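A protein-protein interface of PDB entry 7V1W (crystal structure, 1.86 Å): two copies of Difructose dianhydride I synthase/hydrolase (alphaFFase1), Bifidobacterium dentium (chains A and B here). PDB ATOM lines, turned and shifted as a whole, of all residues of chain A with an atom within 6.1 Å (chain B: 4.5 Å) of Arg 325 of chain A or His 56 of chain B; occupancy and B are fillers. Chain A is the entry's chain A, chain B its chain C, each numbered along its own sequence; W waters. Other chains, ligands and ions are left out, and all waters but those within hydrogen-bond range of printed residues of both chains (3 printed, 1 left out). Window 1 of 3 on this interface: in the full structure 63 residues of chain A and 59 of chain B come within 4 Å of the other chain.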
ATOM      1  N   TYR A 253      -6.133   7.202 -16.502  1.00  0.00           N
ATOM      2  CA  TYR A 253      -5.960   8.613 -16.876  1.00  0.00           C
ATOM      3  C   TYR A 253      -5.470   9.352 -15.625  1.00  0.00           C
ATOM      4  O   TYR A 253      -6.030   9.200 -14.550  1.00  0.00           O
ATOM      5  CB  TYR A 253      -7.272   9.108 -17.485  1.00  0.00           C
ATOM      6  CG  TYR A 253      -7.445  10.601 -17.537  1.00  0.00           C
ATOM      7  CD1 TYR A 253      -6.864  11.341 -18.551  1.00  0.00           C
ATOM      8  CD2 TYR A 253      -8.208  11.265 -16.582  1.00  0.00           C
ATOM      9  CE1 TYR A 253      -7.068  12.711 -18.630  1.00  0.00           C
ATOM     10  CE2 TYR A 253      -8.440  12.623 -16.658  1.00  0.00           C
ATOM     11  CZ  TYR A 253      -7.845  13.351 -17.674  1.00  0.00           C
ATOM     12  OH  TYR A 253      -8.051  14.689 -17.774  1.00  0.00           O
ATOM     13  N   VAL A 254      -4.415  10.147 -15.761  1.00  0.00           N
ATOM     14  CA  VAL A 254      -3.853  10.875 -14.587  1.00  0.00           C
ATOM     15  C   VAL A 254      -3.968  12.373 -14.794  1.00  0.00           C
ATOM     16  O   VAL A 254      -3.435  13.090 -13.922  1.00  0.00           O
ATOM     17  CB  VAL A 254      -2.391  10.503 -14.298  1.00  0.00           C
ATOM     18  CG1 VAL A 254      -2.285   9.089 -13.788  1.00  0.00           C
ATOM     19  CG2 VAL A 254      -1.498  10.770 -15.496  1.00  0.00           C
ATOM     20  N   GLY A 255      -4.651  12.831 -15.849  1.00  0.00           N
ATOM     21  CA  GLY A 255      -5.062  14.243 -15.958  1.00  0.00           C
ATOM     22  C   GLY A 255      -4.660  14.917 -17.252  1.00  0.00           C
ATOM     23  O   GLY A 255      -4.355  14.230 -18.262  1.00  0.00           O
ATOM     24  N   CYS A 256      -4.795  16.240 -17.273  1.00  0.00           N
ATOM     25  CA  CYS A 256      -4.674  17.037 -18.500  1.00  0.00           C
ATOM     26  C   CYS A 256      -4.248  18.459 -18.199  1.00  0.00           C
ATOM     27  O   CYS A 256      -4.415  18.915 -17.041  1.00  0.00           O
ATOM     28  CB  CYS A 256      -5.972  17.044 -19.287  1.00  0.00           C
ATOM     29  SG  CYS A 256      -7.321  18.023 -18.562  1.00  0.00           S
ATOM     30  N   ASN A 257      -3.769  19.128 -19.243  1.00  0.00           N
ATOM     31  CA  ASN A 257      -3.761  20.598 -19.318  1.00  0.00           C
ATOM     32  C   ASN A 257      -4.714  20.942 -20.447  1.00  0.00           C
ATOM     33  O   ASN A 257      -4.997  20.050 -21.295  1.00  0.00           O
ATOM     34  CB  ASN A 257      -2.350  21.218 -19.399  1.00  0.00           C
ATOM     35  CG  ASN A 257      -1.508  20.743 -20.564  1.00  0.00           C
ATOM     36  OD1 ASN A 257      -1.901  20.897 -21.730  1.00  0.00           O
ATOM     37  ND2 ASN A 257      -0.350  20.166 -20.257  1.00  0.00           N
ATOM     38  N   ASP A 273     -17.350  17.942 -17.688  1.00  0.00           N
ATOM     39  CA  ASP A 273     -16.551  16.717 -17.938  1.00  0.00           C
ATOM     40  C   ASP A 273     -17.522  15.528 -17.981  1.00  0.00           C
ATOM     41  O   ASP A 273     -18.438  15.483 -17.136  1.00  0.00           O
ATOM     42  CB  ASP A 273     -15.445  16.521 -16.901  1.00  0.00           C
ATOM     43  CG  ASP A 273     -15.906  16.511 -15.454  1.00  0.00           C
ATOM     44  OD1 ASP A 273     -16.485  17.535 -14.997  1.00  0.00           O
ATOM     45  OD2 ASP A 273     -15.743  15.452 -14.829  1.00  0.00           O
ATOM     46  N   ASP A 292     -15.145  23.486 -12.615  1.00  0.00           N
ATOM     47  CA  ASP A 292     -15.445  22.534 -11.512  1.00  0.00           C
ATOM     48  C   ASP A 292     -14.526  21.332 -11.659  1.00  0.00           C
ATOM     49  O   ASP A 292     -13.993  20.845 -10.637  1.00  0.00           O
ATOM     50  CB  ASP A 292     -16.914  22.096 -11.497  1.00  0.00           C
ATOM     51  CG  ASP A 292     -17.886  23.274 -11.448  1.00  0.00           C
ATOM     52  OD1 ASP A 292     -17.423  24.441 -11.239  1.00  0.00           O
ATOM     53  OD2 ASP A 292     -19.087  23.017 -11.654  1.00  0.00           O
ATOM     54  N   TYR A 293     -14.416  20.817 -12.881  1.00  0.00           N
ATOM     55  CA  TYR A 293     -13.501  19.692 -13.198  1.00  0.00           C
ATOM     56  C   TYR A 293     -12.096  20.057 -12.698  1.00  0.00           C
ATOM     57  O   TYR A 293     -11.420  19.226 -12.066  1.00  0.00           O
ATOM     58  CB  TYR A 293     -13.448  19.399 -14.695  1.00  0.00           C
ATOM     59  CG  TYR A 293     -12.394  18.378 -15.015  1.00  0.00           C
ATOM     60  CD1 TYR A 293     -12.485  17.096 -14.499  1.00  0.00           C
ATOM     61  CD2 TYR A 293     -11.278  18.701 -15.768  1.00  0.00           C
ATOM     62  CE1 TYR A 293     -11.476  16.163 -14.703  1.00  0.00           C
ATOM     63  CE2 TYR A 293     -10.277  17.771 -16.006  1.00  0.00           C
ATOM     64  CZ  TYR A 293     -10.381  16.494 -15.478  1.00  0.00           C
ATOM     65  OH  TYR A 293      -9.406  15.574 -15.708  1.00  0.00           O
ATOM     66  N   PHE A 294     -11.670  21.285 -12.961  1.00  0.00           N
ATOM     67  CA  PHE A 294     -10.362  21.834 -12.512  1.00  0.00           C
ATOM     68  C   PHE A 294     -10.352  22.222 -11.025  1.00  0.00           C
ATOM     69  O   PHE A 294      -9.295  22.748 -10.571  1.00  0.00           O
ATOM     70  CB  PHE A 294      -9.945  22.975 -13.437  1.00  0.00           C
ATOM     71  CG  PHE A 294      -9.608  22.483 -14.827  1.00  0.00           C
ATOM     72  CD1 PHE A 294      -8.553  21.605 -15.033  1.00  0.00           C
ATOM     73  CD2 PHE A 294     -10.328  22.912 -15.937  1.00  0.00           C
ATOM     74  CE1 PHE A 294      -8.271  21.118 -16.299  1.00  0.00           C
ATOM     75  CE2 PHE A 294     -10.049  22.414 -17.198  1.00  0.00           C
ATOM     76  CZ  PHE A 294      -9.013  21.529 -17.375  1.00  0.00           C
ATOM     77  N   ASN A 295     -11.446  21.966 -10.294  1.00  0.00           N
ATOM     78  CA  ASN A 295     -11.567  22.125  -8.818  1.00  0.00           C
ATOM     79  C   ASN A 295     -11.461  23.611  -8.421  1.00  0.00           C
ATOM     80  O   ASN A 295     -11.124  23.887  -7.274  1.00  0.00           O
ATOM     81  CB  ASN A 295     -10.579  21.231  -8.064  1.00  0.00           C
ATOM     82  CG  ASN A 295     -11.074  19.807  -7.850  1.00  0.00           C
ATOM     83  OD1 ASN A 295     -11.173  19.337  -6.712  1.00  0.00           O
ATOM     84  ND2 ASN A 295     -11.350  19.115  -8.946  1.00  0.00           N
ATOM     85  N   PHE A 307      -2.684  19.437  -7.155  1.00  0.00           N
ATOM     86  CA  PHE A 307      -3.430  18.504  -8.042  1.00  0.00           C
ATOM     87  C   PHE A 307      -4.238  19.251  -9.111  1.00  0.00           C
ATOM     88  O   PHE A 307      -4.811  18.610 -10.025  1.00  0.00           O
ATOM     89  CB  PHE A 307      -4.273  17.541  -7.229  1.00  0.00           C
ATOM     90  CG  PHE A 307      -3.500  16.688  -6.262  1.00  0.00           C
ATOM     91  CD1 PHE A 307      -2.439  15.893  -6.689  1.00  0.00           C
ATOM     92  CD2 PHE A 307      -3.825  16.682  -4.914  1.00  0.00           C
ATOM     93  CE1 PHE A 307      -1.764  15.074  -5.793  1.00  0.00           C
ATOM     94  CE2 PHE A 307      -3.112  15.901  -4.015  1.00  0.00           C
ATOM     95  CZ  PHE A 307      -2.089  15.091  -4.455  1.00  0.00           C
ATOM     96  N   PHE A 308      -4.269  20.574  -9.080  1.00  0.00           N
ATOM     97  CA  PHE A 308      -5.138  21.308 -10.029  1.00  0.00           C
ATOM     98  C   PHE A 308      -4.883  22.804  -9.967  1.00  0.00           C
ATOM     99  O   PHE A 308      -4.403  23.268  -8.911  1.00  0.00           O
ATOM    100  CB  PHE A 308      -6.611  21.022  -9.734  1.00  0.00           C
ATOM    101  CG  PHE A 308      -7.055  21.399  -8.349  1.00  0.00           C
ATOM    102  CD1 PHE A 308      -7.460  22.698  -8.067  1.00  0.00           C
ATOM    103  CD2 PHE A 308      -7.105  20.452  -7.332  1.00  0.00           C
ATOM    104  CE1 PHE A 308      -7.874  23.045  -6.786  1.00  0.00           C
ATOM    105  CE2 PHE A 308      -7.560  20.797  -6.065  1.00  0.00           C
ATOM    106  CZ  PHE A 308      -7.904  22.094  -5.784  1.00  0.00           C
ATOM    107  N   GLY A 309      -5.245  23.505 -11.043  1.00  0.00           N
ATOM    108  CA  GLY A 309      -5.419  24.967 -11.026  1.00  0.00           C
ATOM    109  C   GLY A 309      -5.140  25.661 -12.347  1.00  0.00           C
ATOM    110  O   GLY A 309      -5.384  25.123 -13.468  1.00  0.00           O
ATOM    111  N   SER A 323      -5.202  25.698 -17.930  1.00  0.00           N
ATOM    112  CA  SER A 323      -5.600  25.016 -16.676  1.00  0.00           C
ATOM    113  C   SER A 323      -5.025  23.596 -16.658  1.00  0.00           C
ATOM    114  O   SER A 323      -4.593  23.118 -17.724  1.00  0.00           O
ATOM    115  CB  SER A 323      -7.082  25.012 -16.532  1.00  0.00           C
ATOM    116  OG  SER A 323      -7.610  26.296 -16.830  1.00  0.00           O
ATOM    117  N   TYR A 324      -4.958  22.973 -15.490  1.00  0.00           N
ATOM    118  CA  TYR A 324      -4.497  21.568 -15.333  1.00  0.00           C
ATOM    119  C   TYR A 324      -5.254  20.905 -14.194  1.00  0.00           C
ATOM    120  O   TYR A 324      -5.682  21.553 -13.215  1.00  0.00           O
ATOM    121  CB  TYR A 324      -2.998  21.508 -15.055  1.00  0.00           C
ATOM    122  CG  TYR A 324      -2.580  22.079 -13.721  1.00  0.00           C
ATOM    123  CD1 TYR A 324      -2.347  23.439 -13.580  1.00  0.00           C
ATOM    124  CD2 TYR A 324      -2.382  21.269 -12.613  1.00  0.00           C
ATOM    125  CE1 TYR A 324      -1.995  23.987 -12.362  1.00  0.00           C
ATOM    126  CE2 TYR A 324      -2.025  21.796 -11.381  1.00  0.00           C
ATOM    127  CZ  TYR A 324      -1.787  23.156 -11.275  1.00  0.00           C
ATOM    128  OH  TYR A 324      -1.410  23.685 -10.086  1.00  0.00           O
ATOM    129  N   ARG A 325      -5.405  19.603 -14.307  1.00  0.00           N
ATOM    130  CA  ARG A 325      -5.761  18.727 -13.174  1.00  0.00           C
ATOM    131  C   ARG A 325      -4.956  17.431 -13.275  1.00  0.00           C
ATOM    132  O   ARG A 325      -4.850  16.867 -14.391  1.00  0.00           O
ATOM    133  CB  ARG A 325      -7.247  18.416 -13.149  1.00  0.00           C
ATOM    134  CG  ARG A 325      -7.584  17.423 -12.050  1.00  0.00           C
ATOM    135  CD  ARG A 325      -9.019  17.516 -11.663  1.00  0.00           C
ATOM    136  NE  ARG A 325      -9.301  16.457 -10.750  1.00  0.00           N
ATOM    137  CZ  ARG A 325     -10.518  15.996 -10.514  1.00  0.00           C
ATOM    138  NH1 ARG A 325     -11.553  16.553 -11.126  1.00  0.00           N
ATOM    139  NH2 ARG A 325     -10.690  15.018  -9.633  1.00  0.00           N
ATOM    140  N   TRP A 326      -4.412  16.996 -12.148  1.00  0.00           N
ATOM    141  CA  TRP A 326      -3.701  15.709 -11.989  1.00  0.00           C
ATOM    142  C   TRP A 326      -4.578  14.769 -11.162  1.00  0.00           C
ATOM    143  O   TRP A 326      -5.017  15.164 -10.073  1.00  0.00           O
ATOM    144  CB  TRP A 326      -2.352  15.912 -11.323  1.00  0.00           C
ATOM    145  CG  TRP A 326      -1.550  16.974 -11.995  1.00  0.00           C
ATOM    146  CD1 TRP A 326      -0.975  18.047 -11.393  1.00  0.00           C
ATOM    147  CD2 TRP A 326      -1.247  17.071 -13.391  1.00  0.00           C
ATOM    148  NE1 TRP A 326      -0.307  18.801 -12.316  1.00  0.00           N
ATOM    149  CE2 TRP A 326      -0.499  18.250 -13.557  1.00  0.00           C
ATOM    150  CE3 TRP A 326      -1.557  16.302 -14.518  1.00  0.00           C
ATOM    151  CZ2 TRP A 326      -0.007  18.646 -14.791  1.00  0.00           C
ATOM    152  CZ3 TRP A 326      -1.101  16.709 -15.748  1.00  0.00           C
ATOM    153  CH2 TRP A 326      -0.327  17.864 -15.876  1.00  0.00           C
ATOM    154  N   HIS A 327      -4.844  13.579 -11.695  1.00  0.00           N
ATOM    155  CA  HIS A 327      -5.539  12.493 -10.970  1.00  0.00           C
ATOM    156  C   HIS A 327      -4.488  11.511 -10.426  1.00  0.00           C
ATOM    157  O   HIS A 327      -4.384  10.379 -10.948  1.00  0.00           O
ATOM    158  CB  HIS A 327      -6.597  11.832 -11.865  1.00  0.00           C
ATOM    159  CG  HIS A 327      -7.698  12.730 -12.328  1.00  0.00           C
ATOM    160  ND1 HIS A 327      -8.974  12.668 -11.813  1.00  0.00           N
ATOM    161  CD2 HIS A 327      -7.735  13.659 -13.307  1.00  0.00           C
ATOM    162  CE1 HIS A 327      -9.747  13.541 -12.434  1.00  0.00           C
ATOM    163  NE2 HIS A 327      -9.007  14.165 -13.357  1.00  0.00           N
ATOM    164  N   ASP A 330      -6.499   9.897  -7.306  1.00  0.00           N
ATOM    165  CA  ASP A 330      -7.902   9.713  -7.784  1.00  0.00           C
ATOM    166  C   ASP A 330      -7.883   9.447  -9.282  1.00  0.00           C
ATOM    167  O   ASP A 330      -8.594  10.100 -10.038  1.00  0.00           O
ATOM    168  CB  ASP A 330      -8.819  10.922  -7.480  1.00  0.00           C
ATOM    169  CG  ASP A 330      -8.340  12.256  -8.031  1.00  0.00           C
ATOM    170  OD1 ASP A 330      -7.116  12.423  -8.139  1.00  0.00           O
ATOM    171  OD2 ASP A 330      -9.200  13.124  -8.342  1.00  0.00           O
ATOM    172  N   ILE B  54     -13.689   6.431  -1.171  1.00  0.00           N
ATOM    173  CA  ILE B  54     -13.791   7.838  -1.645  1.00  0.00           C
ATOM    174  C   ILE B  54     -12.346   8.309  -1.879  1.00  0.00           C
ATOM    175  O   ILE B  54     -11.538   8.107  -0.989  1.00  0.00           O
ATOM    176  CB  ILE B  54     -14.516   8.740  -0.622  1.00  0.00           C
ATOM    177  CG1 ILE B  54     -15.873   8.180  -0.170  1.00  0.00           C
ATOM    178  CG2 ILE B  54     -14.637  10.136  -1.187  1.00  0.00           C
ATOM    179  CD1 ILE B  54     -16.923   8.179  -1.228  1.00  0.00           C
ATOM    180  N   THR B  55     -12.056   8.885  -3.033  1.00  0.00           N
ATOM    181  CA  THR B  55     -10.700   9.341  -3.433  1.00  0.00           C
ATOM    182  C   THR B  55     -10.598  10.864  -3.512  1.00  0.00           C
ATOM    183  O   THR B  55      -9.473  11.385  -3.425  1.00  0.00           O
ATOM    184  CB  THR B  55     -10.336   8.758  -4.800  1.00  0.00           C
ATOM    185  OG1 THR B  55     -11.292   9.193  -5.784  1.00  0.00           O
ATOM    186  CG2 THR B  55     -10.251   7.252  -4.717  1.00  0.00           C
ATOM    187  N   HIS B  56     -11.709  11.557  -3.719  1.00  0.00           N
ATOM    188  CA  HIS B  56     -11.697  13.006  -4.015  1.00  0.00           C
ATOM    189  C   HIS B  56     -13.093  13.570  -3.802  1.00  0.00           C
ATOM    190  O   HIS B  56     -14.083  12.926  -4.183  1.00  0.00           O
ATOM    191  CB  HIS B  56     -11.137  13.239  -5.432  1.00  0.00           C
ATOM    192  CG  HIS B  56     -11.468  14.576  -5.989  1.00  0.00           C
ATOM    193  ND1 HIS B  56     -12.539  14.771  -6.829  1.00  0.00           N
ATOM    194  CD2 HIS B  56     -10.904  15.785  -5.772  1.00  0.00           C
ATOM    195  CE1 HIS B  56     -12.607  16.041  -7.147  1.00  0.00           C
ATOM    196  NE2 HIS B  56     -11.620  16.697  -6.488  1.00  0.00           N
ATOM    197  N   MET B  57     -13.178  14.718  -3.160  1.00  0.00           N
ATOM    198  CA  MET B  57     -14.422  15.516  -3.087  1.00  0.00           C
ATOM    199  C   MET B  57     -14.093  16.931  -3.542  1.00  0.00           C
ATOM    200  O   MET B  57     -13.052  17.489  -3.076  1.00  0.00           O
ATOM    201  CB  MET B  57     -14.984  15.574  -1.669  1.00  0.00           C
ATOM    202  CG  MET B  57     -15.585  14.295  -1.179  1.00  0.00           C
ATOM    203  SD  MET B  57     -16.241  14.516   0.511  1.00  0.00           S
ATOM    204  CE  MET B  57     -16.932  12.893   0.795  1.00  0.00           C
ATOM    205  N   TRP B  58     -14.933  17.474  -4.419  1.00  0.00           N
ATOM    206  CA  TRP B  58     -14.990  18.912  -4.772  1.00  0.00           C
ATOM    207  C   TRP B  58     -16.408  19.399  -4.491  1.00  0.00           C
ATOM    208  O   TRP B  58     -17.374  18.653  -4.769  1.00  0.00           O
ATOM    209  CB  TRP B  58     -14.584  19.145  -6.235  1.00  0.00           C
ATOM    210  CG  TRP B  58     -14.882  20.534  -6.705  1.00  0.00           C
ATOM    211  CD1 TRP B  58     -14.061  21.627  -6.625  1.00  0.00           C
ATOM    212  CD2 TRP B  58     -16.117  20.995  -7.280  1.00  0.00           C
ATOM    213  NE1 TRP B  58     -14.688  22.727  -7.143  1.00  0.00           N
ATOM    214  CE2 TRP B  58     -15.951  22.374  -7.554  1.00  0.00           C
ATOM    215  CE3 TRP B  58     -17.315  20.366  -7.650  1.00  0.00           C
ATOM    216  CZ2 TRP B  58     -16.963  23.145  -8.139  1.00  0.00           C
ATOM    217  CZ3 TRP B  58     -18.319  21.128  -8.209  1.00  0.00           C
ATOM    218  CH2 TRP B  58     -18.149  22.501  -8.441  1.00  0.00           C
ATOM    219  N   CYS B 162     -11.196  17.932  -1.004  1.00  0.00           N
ATOM    220  CA  CYS B 162     -10.684  16.960  -0.027  1.00  0.00           C
ATOM    221  C   CYS B 162     -10.092  15.762  -0.775  1.00  0.00           C
ATOM    222  O   CYS B 162     -10.806  15.145  -1.608  1.00  0.00           O
ATOM    223  CB  CYS B 162     -11.803  16.530   0.905  1.00  0.00           C
ATOM    224  SG  CYS B 162     -11.210  15.381   2.160  1.00  0.00           S
ATOM    225  N   TYR B 163      -8.869  15.386  -0.424  1.00  0.00           N
ATOM    226  CA  TYR B 163      -8.149  14.230  -0.999  1.00  0.00           C
ATOM    227  C   TYR B 163      -7.848  13.217   0.095  1.00  0.00           C
ATOM    228  O   TYR B 163      -7.121  12.261  -0.216  1.00  0.00           O
ATOM    229  CB  TYR B 163      -6.858  14.700  -1.672  1.00  0.00           C
ATOM    230  CG  TYR B 163      -7.068  15.345  -3.015  1.00  0.00           C
ATOM    231  CD1 TYR B 163      -7.138  14.571  -4.154  1.00  0.00           C
ATOM    232  CD2 TYR B 163      -7.285  16.707  -3.134  1.00  0.00           C
ATOM    233  CE1 TYR B 163      -7.364  15.135  -5.394  1.00  0.00           C
ATOM    234  CE2 TYR B 163      -7.498  17.291  -4.370  1.00  0.00           C
ATOM    235  CZ  TYR B 163      -7.537  16.503  -5.511  1.00  0.00           C
ATOM    236  OH  TYR B 163      -7.752  17.030  -6.754  1.00  0.00           O
ATOM    237  N   ASN B 189     -18.849  17.127  -6.724  1.00  0.00           N
ATOM    238  CA  ASN B 189     -18.274  15.939  -7.406  1.00  0.00           C
ATOM    239  C   ASN B 189     -17.573  15.119  -6.329  1.00  0.00           C
ATOM    240  O   ASN B 189     -16.574  15.624  -5.756  1.00  0.00           O
ATOM    241  CB  ASN B 189     -17.225  16.282  -8.473  1.00  0.00           C
ATOM    242  CG  ASN B 189     -17.718  17.073  -9.666  1.00  0.00           C
ATOM    243  OD1 ASN B 189     -18.851  16.934 -10.089  1.00  0.00           O
ATOM    244  ND2 ASN B 189     -16.832  17.853 -10.270  1.00  0.00           N
ATOM    245  N   ILE B 190     -18.081  13.930  -6.042  1.00  0.00           N
ATOM    246  CA  ILE B 190     -17.515  12.957  -5.059  1.00  0.00           C
ATOM    247  C   ILE B 190     -17.046  11.701  -5.813  1.00  0.00           C
ATOM    248  O   ILE B 190     -17.882  10.899  -6.297  1.00  0.00           O
ATOM    249  CB  ILE B 190     -18.539  12.621  -3.960  1.00  0.00           C
ATOM    250  CG1 ILE B 190     -18.972  13.869  -3.190  1.00  0.00           C
ATOM    251  CG2 ILE B 190     -17.977  11.564  -3.037  1.00  0.00           C
ATOM    252  CD1 ILE B 190     -20.250  13.698  -2.396  1.00  0.00           C
ATOM    253  N   ASP B 191     -15.744  11.542  -5.943  1.00  0.00           N
ATOM    254  CA  ASP B 191     -15.142  10.473  -6.763  1.00  0.00           C
ATOM    255  C   ASP B 191     -14.786   9.321  -5.825  1.00  0.00           C
ATOM    256  O   ASP B 191     -14.395   9.570  -4.662  1.00  0.00           O
ATOM    257  CB  ASP B 191     -13.976  11.010  -7.596  1.00  0.00           C
ATOM    258  CG  ASP B 191     -14.379  12.047  -8.631  1.00  0.00           C
ATOM    259  OD1 ASP B 191     -14.799  11.647  -9.747  1.00  0.00           O
ATOM    260  OD2 ASP B 191     -14.230  13.244  -8.334  1.00  0.00           O
HETATM  261  O   HOH W   1      -7.422  15.291  -8.756  1.00  0.00           O
HETATM  262  O   HOH W   2     -13.627  14.502 -10.475  1.00  0.00           O
HETATM  263  O   HOH W   3     -15.192  16.193 -12.069  1.00  0.00           O
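No position is printed for both chains.
Of the 9 pairs that touch across the chains among the printed residues, none has its exchanged pair printed and touching as well.
Hydrophobic or aromatic side chains of chain A that line the printed part of chain B: Phe 307 and Phe 308.
Of the 10 printed residues of chain B, 4 touch a printed residue of chain A.
Printed residues of chain B that touch a printed residue of chain A: Thr 55, His 56, Trp 58 and Tyr 163.
Hydrophobic or aromatic side chains of chain B that line the printed part of chain A: His 56, Trp 58 and Tyr 163.
Among the printed residues, no Asp or Glu carboxylate lies within 4 Å of a Lys or Arg side-chain nitrogen of the other chain.
Water W2 lies within hydrogen-bond range of the side-chain carboxylate (OD2) of Asp 191 of chain B (2.6 Å) and the guanidinium group (NH1) of Arg 325 of chain A (3.0 Å).
Water W1 lies within hydrogen-bond range of the side-chain hydroxyl (OH) of Tyr 163 of chain B (2.7 Å), the backbone carbonyl oxygen (O) of Trp 326 of chain A (2.7 Å), the side-chain carboxylate (OD2) of Asp 330 of chain A (2.8 Å) and the guanidinium group (NE) of Arg 325 of chain A (3.0 Å).
Water W3 lies within hydrogen-bond range of OD2 of Asp 273 of chain A (2.9 Å) and ND2 of Asn 189 of chain B (2.9 Å).
NH2 of Arg 325 of chain A sits close to ND1 of His 56 of chain B, 3.4 Å away.
A ring nitrogen (NE2) of His 56 of chain B sits at hydrogen-bond distance from the side-chain amide oxygen of Asn 295 of chain A (2.7 Å).
Asp 292 of chain A touches Trp 58 of chain B.
Asn 295 of chain A touches Trp 58 of chain B.
Phe 307 of chain A touches Tyr 163 of chain B.
Tyr 163 of chain B touches Phe 308 of chain A (OH to CD2, 3.5 Å).
Thr 55 of chain B touches Asp 330 of chain A (OG1 to CB, 3.5 Å).
His 56 of chain B touches Asp 330 of chain A.
Tyr 163 of chain B touches Asp 330 of chain A (CE1 to OD1, 3.9 Å).
Cys 256 of chain A touches none of the printed residues of chain B.
Printed residues of chain B within 4 Å of Asp 292 of chain A: Trp 58.
Of the printed residues of chain B, Phe 308 of chain A touches Tyr 163.
Arg 325 of chain A touches one residue of chain B.
Trp 326 of chain A touches none of the printed residues of chain B.
Of the printed residues of chain A, Thr 55 of chain B touches Asp 330 (3.5 Å).
Of chain A, only Asn 295 (2.7 Å), Arg 325 (3.3 Å) and Asp 330 (3.5 Å) come within 4 Å of His 56 of chain B.
Printed residues of chain A within 4 Å of Trp 58 of chain B: Asp 292 (3.1 Å) and Asn 295 (3.4 Å).
The nearest printed residue of chain A that does not touch Tyr 163 of chain B is Asn 295 of chain A (4.1 Å).
The backbone carbonyl oxygen of Tyr 293 of chain A lies within hydrogen-bond range of the side-chain amide nitrogen of Asn 295 of chain A, at 3.1 Å.
A ring nitrogen (NE2) of His 327 of chain A sits close to the guanidinium group of Arg 325 of chain A, at 3.5 Å.
The backbone carbonyl oxygen of Arg 325 of chain A is in hydrogen-bond range of the backbone NH of Cys 256 of chain A.
The side-chain carboxylate of Asp 191 of chain B sits at hydrogen-bond distance from a ring nitrogen (ND1) of His 56 of chain B, 2.7 Å away.
The backbone carbonyl oxygen (O) of Asp 191 of chain B is in hydrogen-bond range of the backbone NH (N) of Thr 55 of chain B.
O of Phe 308 of chain A sits at hydrogen-bond distance from OH of Tyr 324 of chain A, 3.2 Å away.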
